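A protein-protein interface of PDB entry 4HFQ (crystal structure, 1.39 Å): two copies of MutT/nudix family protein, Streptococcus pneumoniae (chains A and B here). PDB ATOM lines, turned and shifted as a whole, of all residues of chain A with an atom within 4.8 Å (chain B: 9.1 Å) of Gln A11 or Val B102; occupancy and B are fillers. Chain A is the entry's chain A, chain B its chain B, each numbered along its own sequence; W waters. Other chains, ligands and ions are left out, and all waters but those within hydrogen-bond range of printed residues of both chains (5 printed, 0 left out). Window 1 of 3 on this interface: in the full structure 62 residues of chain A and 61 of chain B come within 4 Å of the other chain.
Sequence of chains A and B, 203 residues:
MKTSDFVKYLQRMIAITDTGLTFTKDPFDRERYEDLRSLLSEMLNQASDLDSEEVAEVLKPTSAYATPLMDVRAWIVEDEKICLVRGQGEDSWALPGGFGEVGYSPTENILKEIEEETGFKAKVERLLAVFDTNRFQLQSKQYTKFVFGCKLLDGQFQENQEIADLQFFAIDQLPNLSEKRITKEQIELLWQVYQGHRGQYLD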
ATOM      1  N   VAL A   7     -17.125  20.625  11.081  1.00  0.00           N
ATOM      2  CA  VAL A   7     -17.625  20.769   9.713  1.00  0.00           C
ATOM      3  C   VAL A   7     -16.564  21.360   8.789  1.00  0.00           C
ATOM      4  O   VAL A   7     -16.388  20.853   7.677  1.00  0.00           O
ATOM      5  CB  VAL A   7     -18.946  21.569   9.680  1.00  0.00           C
ATOM      6  CG1 VAL A   7     -19.335  21.944   8.258  1.00  0.00           C
ATOM      7  CG2 VAL A   7     -20.055  20.749  10.334  1.00  0.00           C
ATOM      8  N   LYS A   8     -15.846  22.386   9.232  1.00  0.00           N
ATOM      9  CA  LYS A   8     -14.793  22.950   8.409  1.00  0.00           C
ATOM     10  C   LYS A   8     -13.670  21.936   8.141  1.00  0.00           C
ATOM     11  O   LYS A   8     -13.148  21.868   7.024  1.00  0.00           O
ATOM     12  CB  LYS A   8     -14.251  24.226   9.026  1.00  0.00           C
ATOM     13  CG  LYS A   8     -15.230  25.404   8.962  1.00  0.00           C
ATOM     14  CD  LYS A   8     -14.669  26.551   9.802  1.00  0.00           C
ATOM     15  CE  LYS A   8     -15.661  27.665  10.071  1.00  0.00           C
ATOM     16  NZ  LYS A   8     -14.992  28.690  10.911  1.00  0.00           N
ATOM     17  N   TYR A   9     -13.281  21.151   9.151  1.00  0.00           N
ATOM     18  CA  TYR A   9     -12.259  20.107   8.952  1.00  0.00           C
ATOM     19  C   TYR A   9     -12.740  19.081   7.952  1.00  0.00           C
ATOM     20  O   TYR A   9     -11.979  18.724   7.040  1.00  0.00           O
ATOM     21  CB  TYR A   9     -11.940  19.395  10.275  1.00  0.00           C
ATOM     22  CG  TYR A   9     -10.989  20.124  11.197  1.00  0.00           C
ATOM     23  CD1 TYR A   9      -9.708  20.464  10.779  1.00  0.00           C
ATOM     24  CD2 TYR A   9     -11.371  20.468  12.495  1.00  0.00           C
ATOM     25  CE1 TYR A   9      -8.827  21.127  11.610  1.00  0.00           C
ATOM     26  CE2 TYR A   9     -10.498  21.132  13.342  1.00  0.00           C
ATOM     27  CZ  TYR A   9      -9.238  21.473  12.895  1.00  0.00           C
ATOM     28  OH  TYR A   9      -8.334  22.149  13.696  1.00  0.00           O
ATOM     29  N   LEU A  10     -13.978  18.605   8.103  1.00  0.00           N
ATOM     30  CA  LEU A  10     -14.505  17.617   7.170  1.00  0.00           C
ATOM     31  C   LEU A  10     -14.534  18.153   5.734  1.00  0.00           C
ATOM     32  O   LEU A  10     -14.104  17.484   4.781  1.00  0.00           O
ATOM     33  CB  LEU A  10     -15.897  17.152   7.616  1.00  0.00           C
ATOM     34  CG  LEU A  10     -16.659  16.163   6.734  1.00  0.00           C
ATOM     35  CD1 LEU A  10     -15.998  14.802   6.744  1.00  0.00           C
ATOM     36  CD2 LEU A  10     -18.125  16.042   7.142  1.00  0.00           C
ATOM     37  N   GLN A  11     -15.059  19.360   5.596  1.00  0.00           N
ATOM     38  CA  GLN A  11     -15.200  19.996   4.305  1.00  0.00           C
ATOM     39  C   GLN A  11     -13.812  20.095   3.633  1.00  0.00           C
ATOM     40  O   GLN A  11     -13.648  19.764   2.447  1.00  0.00           O
ATOM     41  CB  GLN A  11     -15.843  21.348   4.567  1.00  0.00           C
ATOM     42  CG  GLN A  11     -16.232  22.135   3.352  1.00  0.00           C
ATOM     43  CD  GLN A  11     -16.457  23.579   3.753  1.00  0.00           C
ATOM     44  OE1 GLN A  11     -15.510  24.336   3.947  1.00  0.00           O
ATOM     45  NE2 GLN A  11     -17.743  23.957   3.916  1.00  0.00           N
ATOM     46  N   ARG A  12     -12.802  20.492   4.386  1.00  0.00           N
ATOM     47  CA  ARG A  12     -11.458  20.645   3.856  1.00  0.00           C
ATOM     48  C   ARG A  12     -10.827  19.301   3.468  1.00  0.00           C
ATOM     49  O   ARG A  12     -10.209  19.162   2.397  1.00  0.00           O
ATOM     50  CB  ARG A  12     -10.578  21.406   4.858  1.00  0.00           C
ATOM     51  CG  ARG A  12      -9.164  21.620   4.380  1.00  0.00           C
ATOM     52  CD  ARG A  12      -9.085  22.527   3.162  1.00  0.00           C
ATOM     53  NE  ARG A  12      -7.708  22.602   2.691  1.00  0.00           N
ATOM     54  CZ  ARG A  12      -7.347  22.722   1.419  1.00  0.00           C
ATOM     55  NH1 ARG A  12      -8.252  22.848   0.432  1.00  0.00           N
ATOM     56  NH2 ARG A  12      -6.053  22.713   1.125  1.00  0.00           N
ATOM     57  N   MET A  13     -10.989  18.295   4.325  1.00  0.00           N
ATOM     58  CA  MET A  13     -10.413  16.984   4.018  1.00  0.00           C
ATOM     59  C   MET A  13     -11.066  16.324   2.815  1.00  0.00           C
ATOM     60  O   MET A  13     -10.369  15.683   2.004  1.00  0.00           O
ATOM     61  CB  MET A  13     -10.501  16.081   5.238  1.00  0.00           C
ATOM     62  CG  MET A  13      -9.573  16.549   6.334  1.00  0.00           C
ATOM     63  SD  MET A  13      -9.274  15.365   7.651  1.00  0.00           S
ATOM     64  CE  MET A  13     -10.888  15.373   8.401  1.00  0.00           C
ATOM     65  N   ILE A  14     -12.371  16.521   2.630  1.00  0.00           N
ATOM     66  CA  ILE A  14     -13.020  16.052   1.414  1.00  0.00           C
ATOM     67  C   ILE A  14     -12.372  16.722   0.197  1.00  0.00           C
ATOM     68  O   ILE A  14     -12.027  16.058  -0.784  1.00  0.00           O
ATOM     69  CB  ILE A  14     -14.548  16.302   1.445  1.00  0.00           C
ATOM     70  CG1 ILE A  14     -15.219  15.367   2.466  1.00  0.00           C
ATOM     71  CG2 ILE A  14     -15.149  16.134   0.047  1.00  0.00           C
ATOM     72  CD1 ILE A  14     -16.613  15.789   2.887  1.00  0.00           C
ATOM     73  N   ALA A  15     -12.167  18.032   0.266  1.00  0.00           N
ATOM     74  CA  ALA A  15     -11.589  18.748  -0.859  1.00  0.00           C
ATOM     75  C   ALA A  15     -10.167  18.289  -1.192  1.00  0.00           C
ATOM     76  O   ALA A  15      -9.839  18.097  -2.366  1.00  0.00           O
ATOM     77  CB  ALA A  15     -11.639  20.243  -0.602  1.00  0.00           C
ATOM     78  N   ALA A  66     -12.245  20.424  -6.823  1.00  0.00           N
ATOM     79  CA  ALA A  66     -12.822  20.888  -5.562  1.00  0.00           C
ATOM     80  C   ALA A  66     -12.519  22.365  -5.346  1.00  0.00           C
ATOM     81  O   ALA A  66     -11.409  22.735  -4.999  1.00  0.00           O
ATOM     82  CB  ALA A  66     -12.279  20.057  -4.403  1.00  0.00           C
ATOM     83  N   THR A  67     -13.504  23.211  -5.608  1.00  0.00           N
ATOM     84  CA  THR A  67     -13.375  24.650  -5.365  1.00  0.00           C
ATOM     85  C   THR A  67     -14.629  25.100  -4.626  1.00  0.00           C
ATOM     86  O   THR A  67     -15.650  24.429  -4.648  1.00  0.00           O
ATOM     87  CB  THR A  67     -13.213  25.505  -6.669  1.00  0.00           C
ATOM     88  OG1 THR A  67     -14.471  25.689  -7.319  1.00  0.00           O
ATOM     89  CG2 THR A  67     -12.203  24.881  -7.656  1.00  0.00           C
ATOM     90  N   PRO A  68     -14.589  26.292  -4.021  1.00  0.00           N
ATOM     91  CA  PRO A  68     -15.842  26.893  -3.570  1.00  0.00           C
ATOM     92  C   PRO A  68     -16.827  27.012  -4.736  1.00  0.00           C
ATOM     93  O   PRO A  68     -16.413  27.237  -5.887  1.00  0.00           O
ATOM     94  CB  PRO A  68     -15.396  28.261  -3.043  1.00  0.00           C
ATOM     95  CG  PRO A  68     -13.979  28.058  -2.620  1.00  0.00           C
ATOM     96  CD  PRO A  68     -13.429  27.125  -3.671  1.00  0.00           C
ATOM     97  N   ASN A 134     -18.719  30.189   4.535  1.00  0.00           N
ATOM     98  CA  ASN A 134     -18.108  29.601   5.735  1.00  0.00           C
ATOM     99  C   ASN A 134     -18.065  30.588   6.878  1.00  0.00           C
ATOM    100  O   ASN A 134     -18.083  30.175   8.040  1.00  0.00           O
ATOM    101  CB  ASN A 134     -16.703  29.054   5.453  1.00  0.00           C
ATOM    102  CG  ASN A 134     -16.718  27.650   4.898  1.00  0.00           C
ATOM    103  OD1 ASN A 134     -17.714  27.151   4.395  1.00  0.00           O
ATOM    104  ND2 ASN A 134     -15.554  26.996   4.956  1.00  0.00           N
ATOM    105  N   LEU A 138     -22.267  28.884   7.704  1.00  0.00           N
ATOM    106  CA  LEU A 138     -21.521  27.668   7.479  1.00  0.00           C
ATOM    107  C   LEU A 138     -22.442  26.510   7.116  1.00  0.00           C
ATOM    108  O   LEU A 138     -23.519  26.321   7.710  1.00  0.00           O
ATOM    109  CB  LEU A 138     -20.695  27.325   8.710  1.00  0.00           C
ATOM    110  CG  LEU A 138     -19.833  26.054   8.600  1.00  0.00           C
ATOM    111  CD1 LEU A 138     -18.749  26.158   7.535  1.00  0.00           C
ATOM    112  CD2 LEU A 138     -19.212  25.740   9.959  1.00  0.00           C
ATOM    113  N   GLN A 139     -22.029  25.734   6.122  1.00  0.00           N
ATOM    114  CA  GLN A 139     -22.818  24.612   5.624  1.00  0.00           C
ATOM    115  C   GLN A 139     -21.878  23.621   4.926  1.00  0.00           C
ATOM    116  O   GLN A 139     -20.679  23.903   4.762  1.00  0.00           O
ATOM    117  CB  GLN A 139     -23.959  25.098   4.723  1.00  0.00           C
ATOM    118  CG  GLN A 139     -23.482  26.039   3.620  1.00  0.00           C
ATOM    119  CD  GLN A 139     -24.627  26.717   2.920  1.00  0.00           C
ATOM    120  OE1 GLN A 139     -25.239  26.154   2.027  1.00  0.00           O
ATOM    121  NE2 GLN A 139     -24.926  27.952   3.341  1.00  0.00           N
ATOM    122  N   SER A 140     -22.415  22.479   4.503  1.00  0.00           N
ATOM    123  CA  SER A 140     -21.553  21.392   4.016  1.00  0.00           C
ATOM    124  C   SER A 140     -20.666  21.847   2.858  1.00  0.00           C
ATOM    125  O   SER A 140     -19.471  21.487   2.818  1.00  0.00           O
ATOM    126  CB  SER A 140     -22.374  20.165   3.645  1.00  0.00           C
ATOM    127  OG  SER A 140     -23.341  20.455   2.673  1.00  0.00           O
ATOM    128  N   LYS A 141     -21.218  22.656   1.949  1.00  0.00           N
ATOM    129  CA  LYS A 141     -20.423  23.210   0.862  1.00  0.00           C
ATOM    130  C   LYS A 141     -20.060  24.640   1.162  1.00  0.00           C
ATOM    131  O   LYS A 141     -20.868  25.403   1.694  1.00  0.00           O
ATOM    132  CB  LYS A 141     -21.166  23.160  -0.477  1.00  0.00           C
ATOM    133  CG  LYS A 141     -21.436  21.758  -1.024  1.00  0.00           C
ATOM    134  CD  LYS A 141     -20.149  21.004  -1.337  1.00  0.00           C
ATOM    135  CE  LYS A 141     -20.378  19.691  -2.089  1.00  0.00           C
ATOM    136  NZ  LYS A 141     -21.019  18.627  -1.249  1.00  0.00           N
ATOM    137  N   GLN A 142     -18.846  25.024   0.766  1.00  0.00           N
ATOM    138  CA  GLN A 142     -18.442  26.429   0.769  1.00  0.00           C
ATOM    139  C   GLN A 142     -18.833  27.097  -0.540  1.00  0.00           C
ATOM    140  O   GLN A 142     -18.524  26.581  -1.613  1.00  0.00           O
ATOM    141  CB  GLN A 142     -16.939  26.529   0.983  1.00  0.00           C
ATOM    142  CG  GLN A 142     -16.446  27.965   1.089  1.00  0.00           C
ATOM    143  CD  GLN A 142     -14.969  28.056   1.338  1.00  0.00           C
ATOM    144  OE1 GLN A 142     -14.224  27.189   0.881  1.00  0.00           O
ATOM    145  NE2 GLN A 142     -14.527  29.081   2.070  1.00  0.00           N
ATOM    146  N   ASP B  35      -0.639  18.465   4.399  1.00  0.00           N
ATOM    147  CA  ASP B  35      -1.806  19.258   4.755  1.00  0.00           C
ATOM    148  C   ASP B  35      -2.766  18.399   5.572  1.00  0.00           C
ATOM    149  O   ASP B  35      -3.159  18.765   6.686  1.00  0.00           O
ATOM    150  CB  ASP B  35      -2.431  19.777   3.450  1.00  0.00           C
ATOM    151  CG  ASP B  35      -3.497  20.884   3.638  1.00  0.00           C
ATOM    152  OD1 ASP B  35      -3.858  21.263   4.771  1.00  0.00           O
ATOM    153  OD2 ASP B  35      -3.969  21.352   2.578  1.00  0.00           O
ATOM    154  N   LEU B  36      -3.096  17.219   5.040  1.00  0.00           N
ATOM    155  CA  LEU B  36      -3.956  16.270   5.760  1.00  0.00           C
ATOM    156  C   LEU B  36      -3.396  15.909   7.126  1.00  0.00           C
ATOM    157  O   LEU B  36      -4.139  15.890   8.106  1.00  0.00           O
ATOM    158  CB  LEU B  36      -4.165  14.999   4.947  1.00  0.00           C
ATOM    159  CG  LEU B  36      -5.088  15.133   3.733  1.00  0.00           C
ATOM    160  CD1 LEU B  36      -4.857  13.961   2.786  1.00  0.00           C
ATOM    161  CD2 LEU B  36      -6.550  15.223   4.138  1.00  0.00           C
ATOM    162  N   LEU B  39      -3.879  18.790   9.609  1.00  0.00           N
ATOM    163  CA  LEU B  39      -5.292  18.893  10.008  1.00  0.00           C
ATOM    164  C   LEU B  39      -5.665  17.780  10.993  1.00  0.00           C
ATOM    165  O   LEU B  39      -6.290  18.031  12.031  1.00  0.00           O
ATOM    166  CB  LEU B  39      -6.221  18.848   8.784  1.00  0.00           C
ATOM    167  CG  LEU B  39      -6.063  20.005   7.783  1.00  0.00           C
ATOM    168  CD1 LEU B  39      -6.769  19.659   6.480  1.00  0.00           C
ATOM    169  CD2 LEU B  39      -6.603  21.310   8.363  1.00  0.00           C
ATOM    170  N   MET B  43      -7.020  17.928  14.811  1.00  0.00           N
ATOM    171  CA  MET B  43      -8.270  17.280  15.172  1.00  0.00           C
ATOM    172  C   MET B  43      -8.102  16.327  16.344  1.00  0.00           C
ATOM    173  O   MET B  43      -8.935  16.303  17.250  1.00  0.00           O
ATOM    174  CB  MET B  43      -8.862  16.536  13.980  1.00  0.00           C
ATOM    175  CG  MET B  43      -9.311  17.480  12.855  1.00  0.00           C
ATOM    176  SD  MET B  43      -9.952  16.564  11.444  1.00  0.00           S
ATOM    177  CE  MET B  43     -11.597  16.208  12.061  1.00  0.00           C
ATOM    178  N   VAL B  58     -25.723  22.038  11.000  1.00  0.00           N
ATOM    179  CA  VAL B  58     -24.693  22.859  10.358  1.00  0.00           C
ATOM    180  C   VAL B  58     -24.423  22.395   8.923  1.00  0.00           C
ATOM    181  O   VAL B  58     -24.288  23.216   8.011  1.00  0.00           O
ATOM    182  CB  VAL B  58     -23.415  22.939  11.209  1.00  0.00           C
ATOM    183  CG1 VAL B  58     -22.340  23.741  10.479  1.00  0.00           C
ATOM    184  CG2 VAL B  58     -23.750  23.606  12.525  1.00  0.00           C
ATOM    185  N   LEU B  59     -24.430  21.093   8.693  1.00  0.00           N
ATOM    186  CA  LEU B  59     -24.129  20.572   7.359  1.00  0.00           C
ATOM    187  C   LEU B  59     -25.181  20.935   6.326  1.00  0.00           C
ATOM    188  O   LEU B  59     -24.874  21.132   5.154  1.00  0.00           O
ATOM    189  CB  LEU B  59     -23.954  19.051   7.410  1.00  0.00           C
ATOM    190  CG  LEU B  59     -22.626  18.587   7.996  1.00  0.00           C
ATOM    191  CD1 LEU B  59     -22.703  17.104   8.267  1.00  0.00           C
ATOM    192  CD2 LEU B  59     -21.431  18.886   7.103  1.00  0.00           C
ATOM    193  N   PRO B  61     -27.776  22.886   3.889  1.00  0.00           N
ATOM    194  CA  PRO B  61     -28.314  21.868   2.997  1.00  0.00           C
ATOM    195  C   PRO B  61     -27.234  20.918   2.492  1.00  0.00           C
ATOM    196  O   PRO B  61     -26.066  21.316   2.271  1.00  0.00           O
ATOM    197  CB  PRO B  61     -28.911  22.689   1.848  1.00  0.00           C
ATOM    198  CG  PRO B  61     -28.010  23.880   1.777  1.00  0.00           C
ATOM    199  CD  PRO B  61     -27.734  24.209   3.218  1.00  0.00           C
ATOM    200  N   MET B  70     -13.951  28.004  -9.453  1.00  0.00           N
ATOM    201  CA  MET B  70     -13.311  29.249  -9.016  1.00  0.00           C
ATOM    202  C   MET B  70     -11.850  29.287  -9.441  1.00  0.00           C
ATOM    203  O   MET B  70     -11.081  28.375  -9.137  1.00  0.00           O
ATOM    204  CB  MET B  70     -13.404  29.334  -7.499  1.00  0.00           C
ATOM    205  CG  MET B  70     -12.811  30.609  -6.922  1.00  0.00           C
ATOM    206  SD  MET B  70     -13.051  30.571  -5.137  1.00  0.00           S
ATOM    207  CE  MET B  70     -12.478  32.183  -4.610  1.00  0.00           C
ATOM    208  N   PHE B  99      -6.566  27.688  -9.073  1.00  0.00           N
ATOM    209  CA  PHE B  99      -7.857  27.326  -8.494  1.00  0.00           C
ATOM    210  C   PHE B  99      -8.066  27.907  -7.129  1.00  0.00           C
ATOM    211  O   PHE B  99      -7.161  27.899  -6.297  1.00  0.00           O
ATOM    212  CB  PHE B  99      -7.930  25.813  -8.281  1.00  0.00           C
ATOM    213  CG  PHE B  99      -8.206  25.044  -9.512  1.00  0.00           C
ATOM    214  CD1 PHE B  99      -9.473  25.073 -10.096  1.00  0.00           C
ATOM    215  CD2 PHE B  99      -7.213  24.256 -10.094  1.00  0.00           C
ATOM    216  CE1 PHE B  99      -9.735  24.347 -11.247  1.00  0.00           C
ATOM    217  CE2 PHE B  99      -7.477  23.523 -11.252  1.00  0.00           C
ATOM    218  CZ  PHE B  99      -8.739  23.573 -11.819  1.00  0.00           C
ATOM    219  N   GLY B 100      -9.284  28.376  -6.880  1.00  0.00           N
ATOM    220  CA  GLY B 100      -9.687  28.662  -5.509  1.00  0.00           C
ATOM    221  C   GLY B 100      -9.838  27.348  -4.749  1.00  0.00           C
ATOM    222  O   GLY B 100     -10.435  26.396  -5.272  1.00  0.00           O
ATOM    223  N   GLU B 101      -9.303  27.311  -3.535  1.00  0.00           N
ATOM    224  CA  GLU B 101      -9.379  26.103  -2.702  1.00  0.00           C
ATOM    225  C   GLU B 101     -10.464  26.228  -1.663  1.00  0.00           C
ATOM    226  O   GLU B 101     -10.708  27.305  -1.105  1.00  0.00           O
ATOM    227  CB  GLU B 101      -8.056  25.859  -2.008  1.00  0.00           C
ATOM    228  CG  GLU B 101      -6.928  25.500  -2.960  1.00  0.00           C
ATOM    229  CD  GLU B 101      -5.681  25.223  -2.193  1.00  0.00           C
ATOM    230  OE1 GLU B 101      -5.513  24.069  -1.748  1.00  0.00           O
ATOM    231  OE2 GLU B 101      -4.876  26.165  -2.018  1.00  0.00           O
ATOM    232  N   VAL B 102     -11.078  25.089  -1.370  1.00  0.00           N
ATOM    233  CA  VAL B 102     -12.052  25.008  -0.291  1.00  0.00           C
ATOM    234  C   VAL B 102     -11.342  25.226   1.027  1.00  0.00           C
ATOM    235  O   VAL B 102     -10.251  24.700   1.243  1.00  0.00           O
ATOM    236  CB  VAL B 102     -12.724  23.625  -0.303  1.00  0.00           C
ATOM    237  CG1 VAL B 102     -13.536  23.382   0.979  1.00  0.00           C
ATOM    238  CG2 VAL B 102     -13.582  23.459  -1.546  1.00  0.00           C
ATOM    239  N   GLY B 103     -11.950  26.018   1.906  1.00  0.00           N
ATOM    240  CA  GLY B 103     -11.393  26.306   3.213  1.00  0.00           C
ATOM    241  C   GLY B 103     -10.751  27.669   3.354  1.00  0.00           C
ATOM    242  O   GLY B 103     -10.261  28.032   4.415  1.00  0.00           O
ATOM    243  N   TYR B 104     -10.775  28.445   2.267  1.00  0.00           N
ATOM    244  CA  TYR B 104     -10.172  29.776   2.227  1.00  0.00           C
ATOM    245  C   TYR B 104     -11.189  30.683   1.552  1.00  0.00           C
ATOM    246  O   TYR B 104     -11.885  30.259   0.632  1.00  0.00           O
ATOM    247  CB  TYR B 104      -8.849  29.751   1.425  1.00  0.00           C
ATOM    248  CG  TYR B 104      -7.848  28.784   2.007  1.00  0.00           C
ATOM    249  CD1 TYR B 104      -7.843  27.445   1.627  1.00  0.00           C
ATOM    250  CD2 TYR B 104      -6.947  29.197   2.982  1.00  0.00           C
ATOM    251  CE1 TYR B 104      -6.960  26.540   2.200  1.00  0.00           C
ATOM    252  CE2 TYR B 104      -6.050  28.293   3.549  1.00  0.00           C
ATOM    253  CZ  TYR B 104      -6.077  26.975   3.146  1.00  0.00           C
ATOM    254  OH  TYR B 104      -5.207  26.053   3.708  1.00  0.00           O
ATOM    255  N   SER B 105     -11.236  31.941   2.000  1.00  0.00           N
ATOM    256  CA  SER B 105     -12.105  32.928   1.388  1.00  0.00           C
ATOM    257  C   SER B 105     -11.537  33.388   0.048  1.00  0.00           C
ATOM    258  O   SER B 105     -10.424  33.026  -0.317  1.00  0.00           O
ATOM    259  CB  SER B 105     -12.239  34.127   2.315  1.00  0.00           C
ATOM    260  OG  SER B 105     -11.039  34.884   2.298  1.00  0.00           O
ATOM    261  N   GLU B 108      -8.326  35.276   0.821  1.00  0.00           N
ATOM    262  CA  GLU B 108      -7.327  34.374   1.390  1.00  0.00           C
ATOM    263  C   GLU B 108      -6.779  33.453   0.309  1.00  0.00           C
ATOM    264  O   GLU B 108      -5.594  33.109   0.296  1.00  0.00           O
ATOM    265  CB  GLU B 108      -7.923  33.552   2.521  1.00  0.00           C
ATOM    266  CG  GLU B 108      -8.232  34.364   3.761  1.00  0.00           C
ATOM    267  CD  GLU B 108      -9.108  33.602   4.739  1.00  0.00           C
ATOM    268  OE1 GLU B 108      -9.703  32.551   4.395  1.00  0.00           O
ATOM    269  OE2 GLU B 108      -9.223  34.096   5.890  1.00  0.00           O
ATOM    270  N   ASN B 109      -7.626  33.068  -0.633  1.00  0.00           N
ATOM    271  CA  ASN B 109      -7.187  32.241  -1.759  1.00  0.00           C
ATOM    272  C   ASN B 109      -6.125  32.927  -2.606  1.00  0.00           C
ATOM    273  O   ASN B 109      -5.088  32.311  -2.908  1.00  0.00           O
ATOM    274  CB  ASN B 109      -8.354  31.787  -2.619  1.00  0.00           C
ATOM    275  CG  ASN B 109      -8.829  30.408  -2.249  1.00  0.00           C
ATOM    276  OD1 ASN B 109      -8.048  29.462  -2.268  1.00  0.00           O
ATOM    277  ND2 ASN B 109     -10.108  30.272  -1.931  1.00  0.00           N
ATOM    278  N   LYS B 112      -2.865  33.123  -0.607  1.00  0.00           N
ATOM    279  CA  LYS B 112      -2.233  31.798  -0.526  1.00  0.00           C
ATOM    280  C   LYS B 112      -1.503  31.499  -1.837  1.00  0.00           C
ATOM    281  O   LYS B 112      -0.339  31.074  -1.833  1.00  0.00           O
ATOM    282  CB  LYS B 112      -3.284  30.727  -0.228  1.00  0.00           C
ATOM    283  CG  LYS B 112      -2.706  29.338  -0.017  1.00  0.00           C
ATOM    284  CD  LYS B 112      -3.783  28.357   0.401  1.00  0.00           C
ATOM    285  CE  LYS B 112      -3.168  27.044   0.873  1.00  0.00           C
ATOM    286  NZ  LYS B 112      -2.709  26.228  -0.282  1.00  0.00           N
HETATM  287  O   HOH W   1     -24.352  23.475   1.557  1.00  0.00           O
HETATM  288  O   HOH W   2      -5.768  23.152   4.665  1.00  0.00           O
HETATM  289  O   HOH W   3      -9.997  22.718  -2.596  1.00  0.00           O
HETATM  290  O   HOH W   4      -7.178  22.004  -2.256  1.00  0.00           O
HETATM  291  O   HOH W   5     -12.926  30.298   4.406  1.00  0.00           O
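The guanidinium group of Arg A12 is in salt-bridge range of the side-chain carboxylate of Asp B35 (2.9 Å). The guanidinium group (NH2) of Arg A12 lies within salt-bridge range of the side-chain carboxylate (OE1) of Glu B101 (3.2 Å). The guanidinium group (NH1) of Arg A12 lies within hydrogen-bond range of the backbone carbonyl oxygen (O) of Val B102, 2.8 Å away. The side-chain hydroxyl (OG1) of Thr A67 is in hydrogen-bond range of the backbone NH (N) of Met B70 (3.2 Å). The backbone NH (N) of Ser A140 sits at hydrogen-bond distance from the backbone carbonyl oxygen (O) of Leu B59, 2.9 Å away. OG of Ser A140 sits at hydrogen-bond distance from O of Pro B61 (2.9 Å). OE1 of Gln A142 lies within hydrogen-bond range of N of Gly B103, 2.8 Å away. The side-chain amide nitrogen of Gln A142 lies within hydrogen-bond range of the backbone carbonyl oxygen of Tyr B104 (3.2 Å). O of Val B58 lies close to O of Leu A138 (3.2 Å).
The backbone carbonyl oxygen (O) of Gln A139 lies within hydrogen-bond range of the side-chain amide nitrogen (NE2) of Gln A11. O of Met B70 sits at hydrogen-bond distance from N of Gly B100 (2.9 Å). N of Glu B101 sits at hydrogen-bond distance from OD1 of Asn B109, 2.8 Å away. The side-chain amino group (NZ) of Lys B112 is in salt-bridge range of the side-chain carboxylate (OE2) of Glu B101 (2.8 Å). The backbone carbonyl oxygen of Tyr B104 lies within hydrogen-bond range of the side-chain amide nitrogen of Asn B109.
Among the printed residues, merely in contact across the chains: Gln A139 with Val B58, Thr A67 with Gly B100, Gln A142 with Val B102, Gln A139 with Pro B61, Met A13 with Met B43, Pro A68 with Gly B100, Tyr A9 with Met B43, Ala A15 with Val B102, Thr A67 with Val B102, Thr A67 with Phe B99, Pro A68 with Met B70, Pro A68 with Glu B101, Gln A11 with Val B102, Arg A12 with Leu B39, Val A7 with Val B58, Ala A66 with Gly B100, Pro A68 with Val B102, Val A7 with Leu B59, Gln A139 with Leu B59, Arg A12 with Tyr B104, Tyr A9 with Leu B39 and Met A13 with Leu B36.
Gln A11 touches one residue of chain B. Of the printed residues of chain B, Met A13 touches Leu B36 and Met B43. Of the printed residues of chain B, Pro A68 touches Met B70, Gly B100, Glu B101 and Val B102. Printed residues of chain B within 4 Å of Ser A140: Leu B59 (2.9 Å) and Pro B61 (2.9 Å). Printed residues of chain A within 4 Å of Asp B35: Arg A12 (2.9 Å). Of the printed residues of chain A, Leu B36 touches Met A13 (3.96 Å). Ser B105 touches none of the printed residues of chain A. Lys B112 touches none of the printed residues of chain A. The nearest residue of chain B that does not touch Gln A11 is Gly B103 (4.4 Å).
Of the 18 printed residues of chain A, 13 touch a printed residue of chain B. Hydrophobic or aromatic side chains of chain A that line the printed part of chain B: Val A7, Tyr A9, Met A13, Ala A15, Pro A68 and Leu A138. Printed residues of chain B that touch a printed residue of chain A: Asp B35, Leu B36, Leu B39, Met B43, Val B58, Leu B59, Pro B61, Met B70, Phe B99, Gly B100, Glu B101, Val B102, Gly B103 and Tyr B104. Hydrophobic or aromatic side chains of chain B within 4 Å of the printed part of chain A: Leu B36, Leu B39, Met B43, Val B58, Leu B59, Pro B61, Met B70, Phe B99, Val B102 and Tyr B104. Among the printed residues, 31 pairs touch across the chains.
No position is printed for both chains.
Water W2 lies within hydrogen-bond range of the side-chain carboxylate (OD1) of Asp B35, the guanidinium group (NE) of Arg A12 and the side-chain hydroxyl (OH) of Tyr B104. Water W3 lies within hydrogen-bond range of O of Ala A66 (2.8 Å), N of Val B102 (2.9 Å) and NH1 of Arg A12 (3.5 Å). Water W1 lies within hydrogen-bond range of O of Pro B61 (2.8 Å), OE1 of Gln A139 (2.9 Å), N of Lys A141 (3.3 Å) and OG of Ser A140 (3.4 Å). Water W5 lies within hydrogen-bond range of NE2 of Gln A142 (3.1 Å), N of Ser B105 (3.4 Å) and O of Gly B103 (3.5 Å).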
